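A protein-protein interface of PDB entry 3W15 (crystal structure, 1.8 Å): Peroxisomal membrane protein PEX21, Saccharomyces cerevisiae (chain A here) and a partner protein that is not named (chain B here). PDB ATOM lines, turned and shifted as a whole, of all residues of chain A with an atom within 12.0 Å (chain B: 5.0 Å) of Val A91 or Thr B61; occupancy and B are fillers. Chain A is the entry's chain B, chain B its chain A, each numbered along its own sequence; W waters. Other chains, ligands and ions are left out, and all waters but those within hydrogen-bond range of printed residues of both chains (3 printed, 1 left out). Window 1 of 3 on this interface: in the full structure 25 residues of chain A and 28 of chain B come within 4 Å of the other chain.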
ATOM      1  N   SER A  73      22.143  -7.014   5.746  1.00  0.00           N
ATOM      2  CA  SER A  73      21.536  -8.101   4.981  1.00  0.00           C
ATOM      3  C   SER A  73      20.088  -8.326   5.416  1.00  0.00           C
ATOM      4  O   SER A  73      19.645  -9.461   5.625  1.00  0.00           O
ATOM      5  CB  SER A  73      22.363  -9.379   5.134  1.00  0.00           C
ATOM      6  OG  SER A  73      23.715  -9.148   4.781  1.00  0.00           O
ATOM      7  N   GLU A  74      19.359  -7.221   5.548  1.00  0.00           N
ATOM      8  CA  GLU A  74      17.985  -7.223   6.035  1.00  0.00           C
ATOM      9  C   GLU A  74      17.136  -6.224   5.266  1.00  0.00           C
ATOM     10  O   GLU A  74      17.650  -5.243   4.729  1.00  0.00           O
ATOM     11  CB  GLU A  74      17.952  -6.841   7.512  1.00  0.00           C
ATOM     12  CG  GLU A  74      18.457  -7.898   8.467  1.00  0.00           C
ATOM     13  CD  GLU A  74      18.564  -7.387   9.892  1.00  0.00           C
ATOM     14  OE1 GLU A  74      18.289  -6.188  10.137  1.00  0.00           O
ATOM     15  OE2 GLU A  74      18.922  -8.188  10.773  1.00  0.00           O
ATOM     16  N   ASN A  86      13.256 -12.166   7.647  1.00  0.00           N
ATOM     17  CA  ASN A  86      14.165 -12.633   8.691  1.00  0.00           C
ATOM     18  C   ASN A  86      15.221 -11.610   9.085  1.00  0.00           C
ATOM     19  O   ASN A  86      15.714 -10.849   8.248  1.00  0.00           O
ATOM     20  CB  ASN A  86      14.861 -13.928   8.258  1.00  0.00           C
ATOM     21  CG  ASN A  86      13.957 -15.147   8.350  1.00  0.00           C
ATOM     22  OD1 ASN A  86      12.887 -15.104   8.956  1.00  0.00           O
ATOM     23  ND2 ASN A  86      14.395 -16.250   7.747  1.00  0.00           N
ATOM     24  N   ARG A  87      15.549 -11.601  10.374  1.00  0.00           N
ATOM     25  CA  ARG A  87      16.724 -10.904  10.875  1.00  0.00           C
ATOM     26  C   ARG A  87      17.965 -11.636  10.361  1.00  0.00           C
ATOM     27  O   ARG A  87      17.947 -12.860  10.225  1.00  0.00           O
ATOM     28  CB  ARG A  87      16.708 -10.878  12.413  1.00  0.00           C
ATOM     29  CG  ARG A  87      17.975 -10.299  13.051  1.00  0.00           C
ATOM     30  CD  ARG A  87      17.689  -9.573  14.364  1.00  0.00           C
ATOM     31  NE  ARG A  87      16.821  -8.403  14.193  1.00  0.00           N
ATOM     32  CZ  ARG A  87      17.215  -7.221  13.724  1.00  0.00           C
ATOM     33  NH1 ARG A  87      18.479  -7.020  13.360  1.00  0.00           N
ATOM     34  NH2 ARG A  87      16.336  -6.231  13.613  1.00  0.00           N
ATOM     35  N   HIS A  88      19.021 -10.893  10.045  1.00  0.00           N
ATOM     36  CA  HIS A  88      20.292 -11.529   9.720  1.00  0.00           C
ATOM     37  C   HIS A  88      21.150 -11.727  10.964  1.00  0.00           C
ATOM     38  O   HIS A  88      21.372 -10.789  11.744  1.00  0.00           O
ATOM     39  CB  HIS A  88      21.085 -10.768   8.661  1.00  0.00           C
ATOM     40  CG  HIS A  88      22.363 -11.453   8.288  1.00  0.00           C
ATOM     41  ND1 HIS A  88      23.575 -11.129   8.856  1.00  0.00           N
ATOM     42  CD2 HIS A  88      22.602 -12.497   7.458  1.00  0.00           C
ATOM     43  CE1 HIS A  88      24.513 -11.924   8.369  1.00  0.00           C
ATOM     44  NE2 HIS A  88      23.949 -12.760   7.515  1.00  0.00           N
ATOM     45  N   ILE A  89      21.623 -12.957  11.134  1.00  0.00           N
ATOM     46  CA  ILE A  89      22.502 -13.326  12.230  1.00  0.00           C
ATOM     47  C   ILE A  89      23.873 -13.639  11.645  1.00  0.00           C
ATOM     48  O   ILE A  89      23.992 -14.492  10.766  1.00  0.00           O
ATOM     49  CB  ILE A  89      21.945 -14.562  12.990  1.00  0.00           C
ATOM     50  CG1 ILE A  89      20.475 -14.332  13.390  1.00  0.00           C
ATOM     51  CG2 ILE A  89      22.805 -14.887  14.203  1.00  0.00           C
ATOM     52  CD1 ILE A  89      19.736 -15.592  13.847  1.00  0.00           C
ATOM     53  N   PHE A  90      24.899 -12.924  12.106  1.00  0.00           N
ATOM     54  CA  PHE A  90      26.272 -13.190  11.689  1.00  0.00           C
ATOM     55  C   PHE A  90      26.641 -14.654  11.942  1.00  0.00           C
ATOM     56  O   PHE A  90      26.392 -15.181  13.025  1.00  0.00           O
ATOM     57  CB  PHE A  90      27.255 -12.274  12.425  1.00  0.00           C
ATOM     58  CG  PHE A  90      28.701 -12.602  12.156  1.00  0.00           C
ATOM     59  CD1 PHE A  90      29.266 -12.345  10.907  1.00  0.00           C
ATOM     60  CD2 PHE A  90      29.490 -13.187  13.139  1.00  0.00           C
ATOM     61  CE1 PHE A  90      30.600 -12.660  10.647  1.00  0.00           C
ATOM     62  CE2 PHE A  90      30.827 -13.503  12.888  1.00  0.00           C
ATOM     63  CZ  PHE A  90      31.380 -13.245  11.637  1.00  0.00           C
ATOM     64  N   VAL A  91      27.220 -15.302  10.932  1.00  0.00           N
ATOM     65  CA  VAL A  91      27.735 -16.670  11.077  1.00  0.00           C
ATOM     66  C   VAL A  91      29.224 -16.726  10.721  1.00  0.00           C
ATOM     67  O   VAL A  91      29.610 -16.413   9.588  1.00  0.00           O
ATOM     68  CB  VAL A  91      26.952 -17.691  10.200  1.00  0.00           C
ATOM     69  CG1 VAL A  91      27.548 -19.083  10.354  1.00  0.00           C
ATOM     70  CG2 VAL A  91      25.456 -17.707  10.558  1.00  0.00           C
ATOM     71  N   LYS A  92      30.046 -17.135  11.688  1.00  0.00           N
ATOM     72  CA  LYS A  92      31.507 -17.242  11.528  1.00  0.00           C
ATOM     73  C   LYS A  92      31.878 -18.284  10.480  1.00  0.00           C
ATOM     74  O   LYS A  92      31.152 -19.260  10.308  1.00  0.00           O
ATOM     75  CB  LYS A  92      32.154 -17.711  12.833  1.00  0.00           C
ATOM     76  CG  LYS A  92      32.315 -16.684  13.928  1.00  0.00           C
ATOM     77  CD  LYS A  92      33.102 -17.288  15.097  1.00  0.00           C
ATOM     78  CE  LYS A  92      34.577 -17.497  14.747  1.00  0.00           C
ATOM     79  NZ  LYS A  92      35.276 -18.424  15.683  1.00  0.00           N
ATOM     80  N   ASP A  93      33.026 -18.098   9.827  1.00  0.00           N
ATOM     81  CA  ASP A  93      33.599 -19.134   8.954  1.00  0.00           C
ATOM     82  C   ASP A  93      34.362 -20.195   9.756  1.00  0.00           C
ATOM     83  O   ASP A  93      35.431 -20.652   9.340  1.00  0.00           O
ATOM     84  CB  ASP A  93      34.513 -18.520   7.887  1.00  0.00           C
ATOM     85  CG  ASP A  93      33.744 -17.955   6.707  1.00  0.00           C
ATOM     86  OD1 ASP A  93      32.602 -18.391   6.447  1.00  0.00           O
ATOM     87  OD2 ASP A  93      34.298 -17.067   6.025  1.00  0.00           O
ATOM     88  N   GLU A  94      33.804 -20.586  10.902  1.00  0.00           N
ATOM     89  CA  GLU A  94      34.378 -21.637  11.734  1.00  0.00           C
ATOM     90  C   GLU A  94      34.074 -22.998  11.115  1.00  0.00           C
ATOM     91  O   GLU A  94      33.006 -23.197  10.529  1.00  0.00           O
ATOM     92  CB  GLU A  94      33.804 -21.567  13.164  1.00  0.00           C
ATOM     93  CG  GLU A  94      34.462 -22.531  14.179  1.00  0.00           C
ATOM     94  CD  GLU A  94      34.175 -22.166  15.638  1.00  0.00           C
ATOM     95  OE1 GLU A  94      34.141 -20.965  15.961  1.00  0.00           O
ATOM     96  OE2 GLU A  94      33.973 -23.086  16.464  1.00  0.00           O
ATOM     97  N   ILE A  95      35.021 -23.924  11.235  1.00  0.00           N
ATOM     98  CA  ILE A  95      34.738 -25.334  10.963  1.00  0.00           C
ATOM     99  C   ILE A  95      35.140 -26.151  12.180  1.00  0.00           C
ATOM    100  O   ILE A  95      36.071 -25.778  12.893  1.00  0.00           O
ATOM    101  CB  ILE A  95      35.456 -25.900   9.702  1.00  0.00           C
ATOM    102  CG1 ILE A  95      36.975 -25.747   9.803  1.00  0.00           C
ATOM    103  CG2 ILE A  95      34.893 -25.269   8.414  1.00  0.00           C
ATOM    104  CD1 ILE A  95      37.743 -26.853   9.093  1.00  0.00           C
ATOM    105  N   HIS A  96      34.448 -27.262  12.403  1.00  0.00           N
ATOM    106  CA  HIS A  96      34.841 -28.215  13.444  1.00  0.00           C
ATOM    107  C   HIS A  96      36.162 -28.870  13.064  1.00  0.00           C
ATOM    108  O   HIS A  96      36.465 -29.018  11.880  1.00  0.00           O
ATOM    109  CB  HIS A  96      33.771 -29.290  13.612  1.00  0.00           C
ATOM    110  CG  HIS A  96      32.427 -28.749  13.981  1.00  0.00           C
ATOM    111  ND1 HIS A  96      32.151 -28.225  15.224  1.00  0.00           N
ATOM    112  CD2 HIS A  96      31.284 -28.636  13.264  1.00  0.00           C
ATOM    113  CE1 HIS A  96      30.894 -27.819  15.260  1.00  0.00           C
ATOM    114  NE2 HIS A  96      30.346 -28.057  14.083  1.00  0.00           N
ATOM    115  N   ASN B  39      20.478 -14.689   5.747  1.00  0.00           N
ATOM    116  CA  ASN B  39      20.953 -16.044   6.062  1.00  0.00           C
ATOM    117  C   ASN B  39      20.469 -17.121   5.109  1.00  0.00           C
ATOM    118  O   ASN B  39      19.428 -16.993   4.466  1.00  0.00           O
ATOM    119  CB  ASN B  39      20.520 -16.471   7.467  1.00  0.00           C
ATOM    120  CG  ASN B  39      21.205 -15.684   8.556  1.00  0.00           C
ATOM    121  OD1 ASN B  39      20.545 -14.973   9.315  1.00  0.00           O
ATOM    122  ND2 ASN B  39      22.527 -15.802   8.647  1.00  0.00           N
ATOM    123  N   GLY B  40      21.240 -18.199   5.047  1.00  0.00           N
ATOM    124  CA  GLY B  40      20.762 -19.438   4.475  1.00  0.00           C
ATOM    125  C   GLY B  40      20.530 -20.377   5.635  1.00  0.00           C
ATOM    126  O   GLY B  40      20.921 -20.092   6.773  1.00  0.00           O
ATOM    127  N   LYS B  41      19.877 -21.490   5.358  1.00  0.00           N
ATOM    128  CA  LYS B  41      19.644 -22.491   6.381  1.00  0.00           C
ATOM    129  C   LYS B  41      19.482 -23.856   5.760  1.00  0.00           C
ATOM    130  O   LYS B  41      18.747 -24.032   4.775  1.00  0.00           O
ATOM    131  CB  LYS B  41      18.422 -22.130   7.239  1.00  0.00           C
ATOM    132  CG  LYS B  41      18.260 -23.005   8.490  1.00  0.00           C
ATOM    133  CD  LYS B  41      17.339 -22.328   9.501  1.00  0.00           C
ATOM    134  CE  LYS B  41      17.122 -23.195  10.734  1.00  0.00           C
ATOM    135  NZ  LYS B  41      16.258 -22.512  11.754  1.00  0.00           N
ATOM    136  N   PHE B  59      21.302 -25.898  10.387  1.00  0.00           N
ATOM    137  CA  PHE B  59      22.493 -25.076  10.424  1.00  0.00           C
ATOM    138  C   PHE B  59      22.200 -23.761   9.723  1.00  0.00           C
ATOM    139  O   PHE B  59      21.867 -23.749   8.543  1.00  0.00           O
ATOM    140  CB  PHE B  59      23.646 -25.779   9.703  1.00  0.00           C
ATOM    141  CG  PHE B  59      24.011 -27.124  10.284  1.00  0.00           C
ATOM    142  CD1 PHE B  59      23.404 -28.288   9.815  1.00  0.00           C
ATOM    143  CD2 PHE B  59      24.968 -27.219  11.291  1.00  0.00           C
ATOM    144  CE1 PHE B  59      23.747 -29.537  10.341  1.00  0.00           C
ATOM    145  CE2 PHE B  59      25.323 -28.461  11.830  1.00  0.00           C
ATOM    146  CZ  PHE B  59      24.718 -29.624  11.351  1.00  0.00           C
ATOM    147  N   LEU B  60      22.322 -22.659  10.458  1.00  0.00           N
ATOM    148  CA  LEU B  60      22.242 -21.331   9.866  1.00  0.00           C
ATOM    149  C   LEU B  60      23.555 -20.960   9.186  1.00  0.00           C
ATOM    150  O   LEU B  60      24.634 -21.136   9.767  1.00  0.00           O
ATOM    151  CB  LEU B  60      21.925 -20.297  10.948  1.00  0.00           C
ATOM    152  CG  LEU B  60      21.451 -18.948  10.423  1.00  0.00           C
ATOM    153  CD1 LEU B  60      20.000 -19.047   9.998  1.00  0.00           C
ATOM    154  CD2 LEU B  60      21.622 -17.898  11.512  1.00  0.00           C
ATOM    155  N   THR B  61      23.461 -20.444   7.962  1.00  0.00           N
ATOM    156  CA  THR B  61      24.645 -20.009   7.226  1.00  0.00           C
ATOM    157  C   THR B  61      24.583 -18.512   6.969  1.00  0.00           C
ATOM    158  O   THR B  61      23.510 -17.908   7.021  1.00  0.00           O
ATOM    159  CB  THR B  61      24.801 -20.754   5.878  1.00  0.00           C
ATOM    160  OG1 THR B  61      23.640 -20.530   5.068  1.00  0.00           O
ATOM    161  CG2 THR B  61      24.969 -22.259   6.104  1.00  0.00           C
ATOM    162  N   GLN B  62      25.741 -17.929   6.676  1.00  0.00           N
ATOM    163  CA  GLN B  62      25.887 -16.479   6.493  1.00  0.00           C
ATOM    164  C   GLN B  62      25.066 -15.940   5.319  1.00  0.00           C
ATOM    165  O   GLN B  62      24.487 -14.844   5.399  1.00  0.00           O
ATOM    166  CB  GLN B  62      27.375 -16.138   6.319  1.00  0.00           C
ATOM    167  CG  GLN B  62      27.706 -14.655   6.039  1.00  0.00           C
ATOM    168  CD  GLN B  62      27.432 -13.701   7.204  1.00  0.00           C
ATOM    169  OE1 GLN B  62      26.999 -14.097   8.286  1.00  0.00           O
ATOM    170  NE2 GLN B  62      27.685 -12.423   6.967  1.00  0.00           N
ATOM    171  N   ASP B  63      25.029 -16.716   4.233  1.00  0.00           N
ATOM    172  CA  ASP B  63      24.291 -16.359   3.033  1.00  0.00           C
ATOM    173  C   ASP B  63      23.387 -17.508   2.603  1.00  0.00           C
ATOM    174  O   ASP B  63      23.559 -18.659   3.031  1.00  0.00           O
ATOM    175  CB  ASP B  63      25.258 -15.997   1.900  1.00  0.00           C
ATOM    176  CG  ASP B  63      24.594 -15.195   0.773  1.00  0.00           C
ATOM    177  OD1 ASP B  63      23.370 -14.877   0.827  1.00  0.00           O
ATOM    178  OD2 ASP B  63      25.324 -14.881  -0.191  1.00  0.00           O
ATOM    179  N   CYS B  64      22.430 -17.162   1.752  1.00  0.00           N
ATOM    180  CA  CYS B  64      21.407 -18.065   1.249  1.00  0.00           C
ATOM    181  C   CYS B  64      21.998 -19.334   0.645  1.00  0.00           C
ATOM    182  O   CYS B  64      23.071 -19.303   0.019  1.00  0.00           O
ATOM    183  CB  CYS B  64      20.547 -17.331   0.219  1.00  0.00           C
ATOM    184  SG  CYS B  64      19.669 -15.886   0.916  1.00  0.00           S
ATOM    185  N   LEU B  65      21.301 -20.444   0.870  1.00  0.00           N
ATOM    186  CA  LEU B  65      21.677 -21.736   0.290  1.00  0.00           C
ATOM    187  C   LEU B  65      20.828 -22.035  -0.933  1.00  0.00           C
ATOM    188  O   LEU B  65      19.594 -21.900  -0.901  1.00  0.00           O
ATOM    189  CB  LEU B  65      21.548 -22.863   1.321  1.00  0.00           C
ATOM    190  CG  LEU B  65      22.361 -22.704   2.606  1.00  0.00           C
ATOM    191  CD1 LEU B  65      22.193 -23.926   3.513  1.00  0.00           C
ATOM    192  CD2 LEU B  65      23.839 -22.459   2.279  1.00  0.00           C
ATOM    193  N   GLN B  82      26.346 -22.320  -1.550  1.00  0.00           N
ATOM    194  CA  GLN B  82      26.043 -21.049  -0.871  1.00  0.00           C
ATOM    195  C   GLN B  82      26.193 -19.832  -1.791  1.00  0.00           C
ATOM    196  O   GLN B  82      26.945 -19.861  -2.774  1.00  0.00           O
ATOM    197  CB  GLN B  82      26.921 -20.902   0.377  1.00  0.00           C
ATOM    198  CG  GLN B  82      26.512 -19.798   1.355  1.00  0.00           C
ATOM    199  CD  GLN B  82      26.965 -20.103   2.772  1.00  0.00           C
ATOM    200  OE1 GLN B  82      26.838 -21.238   3.231  1.00  0.00           O
ATOM    201  NE2 GLN B  82      27.503 -19.101   3.463  1.00  0.00           N
ATOM    202  N   ARG B  88      29.847 -25.840   1.429  1.00  0.00           N
ATOM    203  CA  ARG B  88      30.148 -26.214   2.806  1.00  0.00           C
ATOM    204  C   ARG B  88      29.617 -27.610   3.064  1.00  0.00           C
ATOM    205  O   ARG B  88      28.496 -27.941   2.685  1.00  0.00           O
ATOM    206  CB  ARG B  88      29.559 -25.176   3.775  1.00  0.00           C
ATOM    207  CG  ARG B  88      30.139 -23.775   3.527  1.00  0.00           C
ATOM    208  CD  ARG B  88      29.535 -22.667   4.384  1.00  0.00           C
ATOM    209  NE  ARG B  88      30.068 -21.378   3.927  1.00  0.00           N
ATOM    210  CZ  ARG B  88      30.819 -20.545   4.649  1.00  0.00           C
ATOM    211  NH1 ARG B  88      31.131 -20.804   5.926  1.00  0.00           N
ATOM    212  NH2 ARG B  88      31.244 -19.422   4.092  1.00  0.00           N
ATOM    213  N   PHE B  90      28.687 -30.473   5.842  1.00  0.00           N
ATOM    214  CA  PHE B  90      28.251 -30.583   7.228  1.00  0.00           C
ATOM    215  C   PHE B  90      28.206 -32.038   7.630  1.00  0.00           C
ATOM    216  O   PHE B  90      27.866 -32.896   6.818  1.00  0.00           O
ATOM    217  CB  PHE B  90      26.851 -29.997   7.390  1.00  0.00           C
ATOM    218  CG  PHE B  90      26.811 -28.505   7.308  1.00  0.00           C
ATOM    219  CD1 PHE B  90      26.965 -27.736   8.456  1.00  0.00           C
ATOM    220  CD2 PHE B  90      26.630 -27.869   6.086  1.00  0.00           C
ATOM    221  CE1 PHE B  90      26.937 -26.347   8.392  1.00  0.00           C
ATOM    222  CE2 PHE B  90      26.600 -26.480   6.006  1.00  0.00           C
ATOM    223  CZ  PHE B  90      26.757 -25.714   7.162  1.00  0.00           C
ATOM    224  N   PHE B  97      28.206 -25.434  12.893  1.00  0.00           N
ATOM    225  CA  PHE B  97      29.235 -25.222  11.877  1.00  0.00           C
ATOM    226  C   PHE B  97      29.459 -26.430  10.989  1.00  0.00           C
ATOM    227  O   PHE B  97      29.129 -27.560  11.366  1.00  0.00           O
ATOM    228  CB  PHE B  97      30.563 -24.811  12.531  1.00  0.00           C
ATOM    229  CG  PHE B  97      30.493 -23.502  13.257  1.00  0.00           C
ATOM    230  CD1 PHE B  97      30.147 -22.338  12.583  1.00  0.00           C
ATOM    231  CD2 PHE B  97      30.796 -23.431  14.612  1.00  0.00           C
ATOM    232  CE1 PHE B  97      30.081 -21.115  13.259  1.00  0.00           C
ATOM    233  CE2 PHE B  97      30.749 -22.221  15.295  1.00  0.00           C
ATOM    234  CZ  PHE B  97      30.383 -21.061  14.620  1.00  0.00           C
HETATM  235  O   HOH W   1      31.255 -21.605   8.943  1.00  0.00           O
HETATM  236  O   HOH W   2      18.381 -13.675   7.353  1.00  0.00           O
HETATM  237  O   HOH W   3      17.994 -15.691  10.028  1.00  0.00           O
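Asn A86 touches none of the printed residues of chain B. Of the printed residues of chain B, His A88 touches Asn B39 and Gln B62. Printed residues of chain B within 4 Å of Phe A90: Gln B62 (3.6 Å). Printed residues of chain B within 4 Å of Val A91: Asn B39 (3.98 Å), Leu B60 (3.6 Å), Thr B61 (3.8 Å) and Gln B62 (2.9 Å). Of the printed residues of chain B, Lys A92 touches Phe B97. Of the printed residues of chain B, Asp A93 touches Arg B88. Of the printed residues of chain B, Glu A94 touches Phe B97 (3.4 Å). No residue of chain A comes within 4 Å of Gly B40. Leu B60 touches two residues of chain A. Thr B61 touches just one residue of chain A: Val A91. Gln B62 touches just these residues of chain A: His A88, Ile A89, Phe A90 and Val A91. No residue of chain A comes within 4 Å of Cys B64. Printed residues of chain A within 4 Å of Arg B88: Asp A93 (2.9 Å). Phe B90 touches none of the printed residues of chain A. The nearest printed residue of chain B that does not touch Val A91 is Phe B97 (4.4 Å).
Among the printed residues, pairs that only touch across the chains: Glu A94 with Phe B97 (3.4 Å), His A88 with Asn B39 (3.5 Å), Phe A90 with Gln B62 (3.6 Å), Val A91 with Leu B60 (3.6 Å), Lys A92 with Phe B97 (3.6 Å), Ile A89 with Leu B60 (3.7 Å), Val A91 with Thr B61 (3.8 Å), Ile A89 with Gln B62 (3.9 Å) and Val A91 with Asn B39 (3.98 Å).
ND2 of Asn B39 lies within hydrogen-bond range of O of Thr B61. O of Asn B39 lies within hydrogen-bond range of SG of Cys B64 (3.7 Å). O of Gly B40 lies within hydrogen-bond range of N of Thr B61 (2.8 Å). The side-chain amide oxygen of Gln B82 sits close to the guanidinium group of Arg B88, 3.3 Å away. The side-chain carboxylate of Glu A74 lies within hydrogen-bond range of the backbone NH of His A88 (2.8 Å). NZ of Lys A92 is in salt-bridge range of OE1 of Glu A94 (2.8 Å).
OD1 of Asn B39 sits close to O of Arg A87, 3.5 Å away. The side-chain amide nitrogen (ND2) of Asn B39 is in hydrogen-bond range of the backbone carbonyl oxygen (O) of Ile A89, 2.9 Å away. O of Gln B62 sits at hydrogen-bond distance from NE2 of His A88 (3.0 Å). The side-chain amide oxygen of Gln B62 lies within hydrogen-bond range of the backbone NH of Val A91 (2.9 Å). NH1 of Arg B88 lies within salt-bridge range of OD1 of Asp A93 (2.9 Å). NE2 of His A96 lies within hydrogen-bond range of O of Phe B97, at 3.0 Å.
Of the 13 printed residues of chain A, 9 touch a printed residue of chain B. Printed residues of chain A that touch a printed residue of chain B: Arg A87, His A88, Ile A89, Phe A90, Val A91, Lys A92, Asp A93, Glu A94 and His A96. Hydrophobic or aromatic side chains of chain A within 4 Å of the printed part of chain B: His A88, Ile A89, Phe A90, Val A91 and His A96. Printed residues of chain B that touch a printed residue of chain A: Asn B39, Leu B60, Thr B61, Gln B62, Arg B88 and Phe B97. Hydrophobic or aromatic side chains of chain B that line the printed part of chain A: Leu B60 and Phe B97.
Water W1 lies within hydrogen-bond range of O of Lys A92 (2.7 Å), O of Glu A94 (2.8 Å) and NH1 of Arg B88 (3.1 Å). Water W3 lies within hydrogen-bond range of the side-chain amide oxygen of Asn B39 and the backbone carbonyl oxygen of Arg A87. Water W2 lies within hydrogen-bond range of the backbone NH (N) of Asn B39 (2.8 Å) and the backbone carbonyl oxygen (O) of Arg A87 (3.0 Å).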
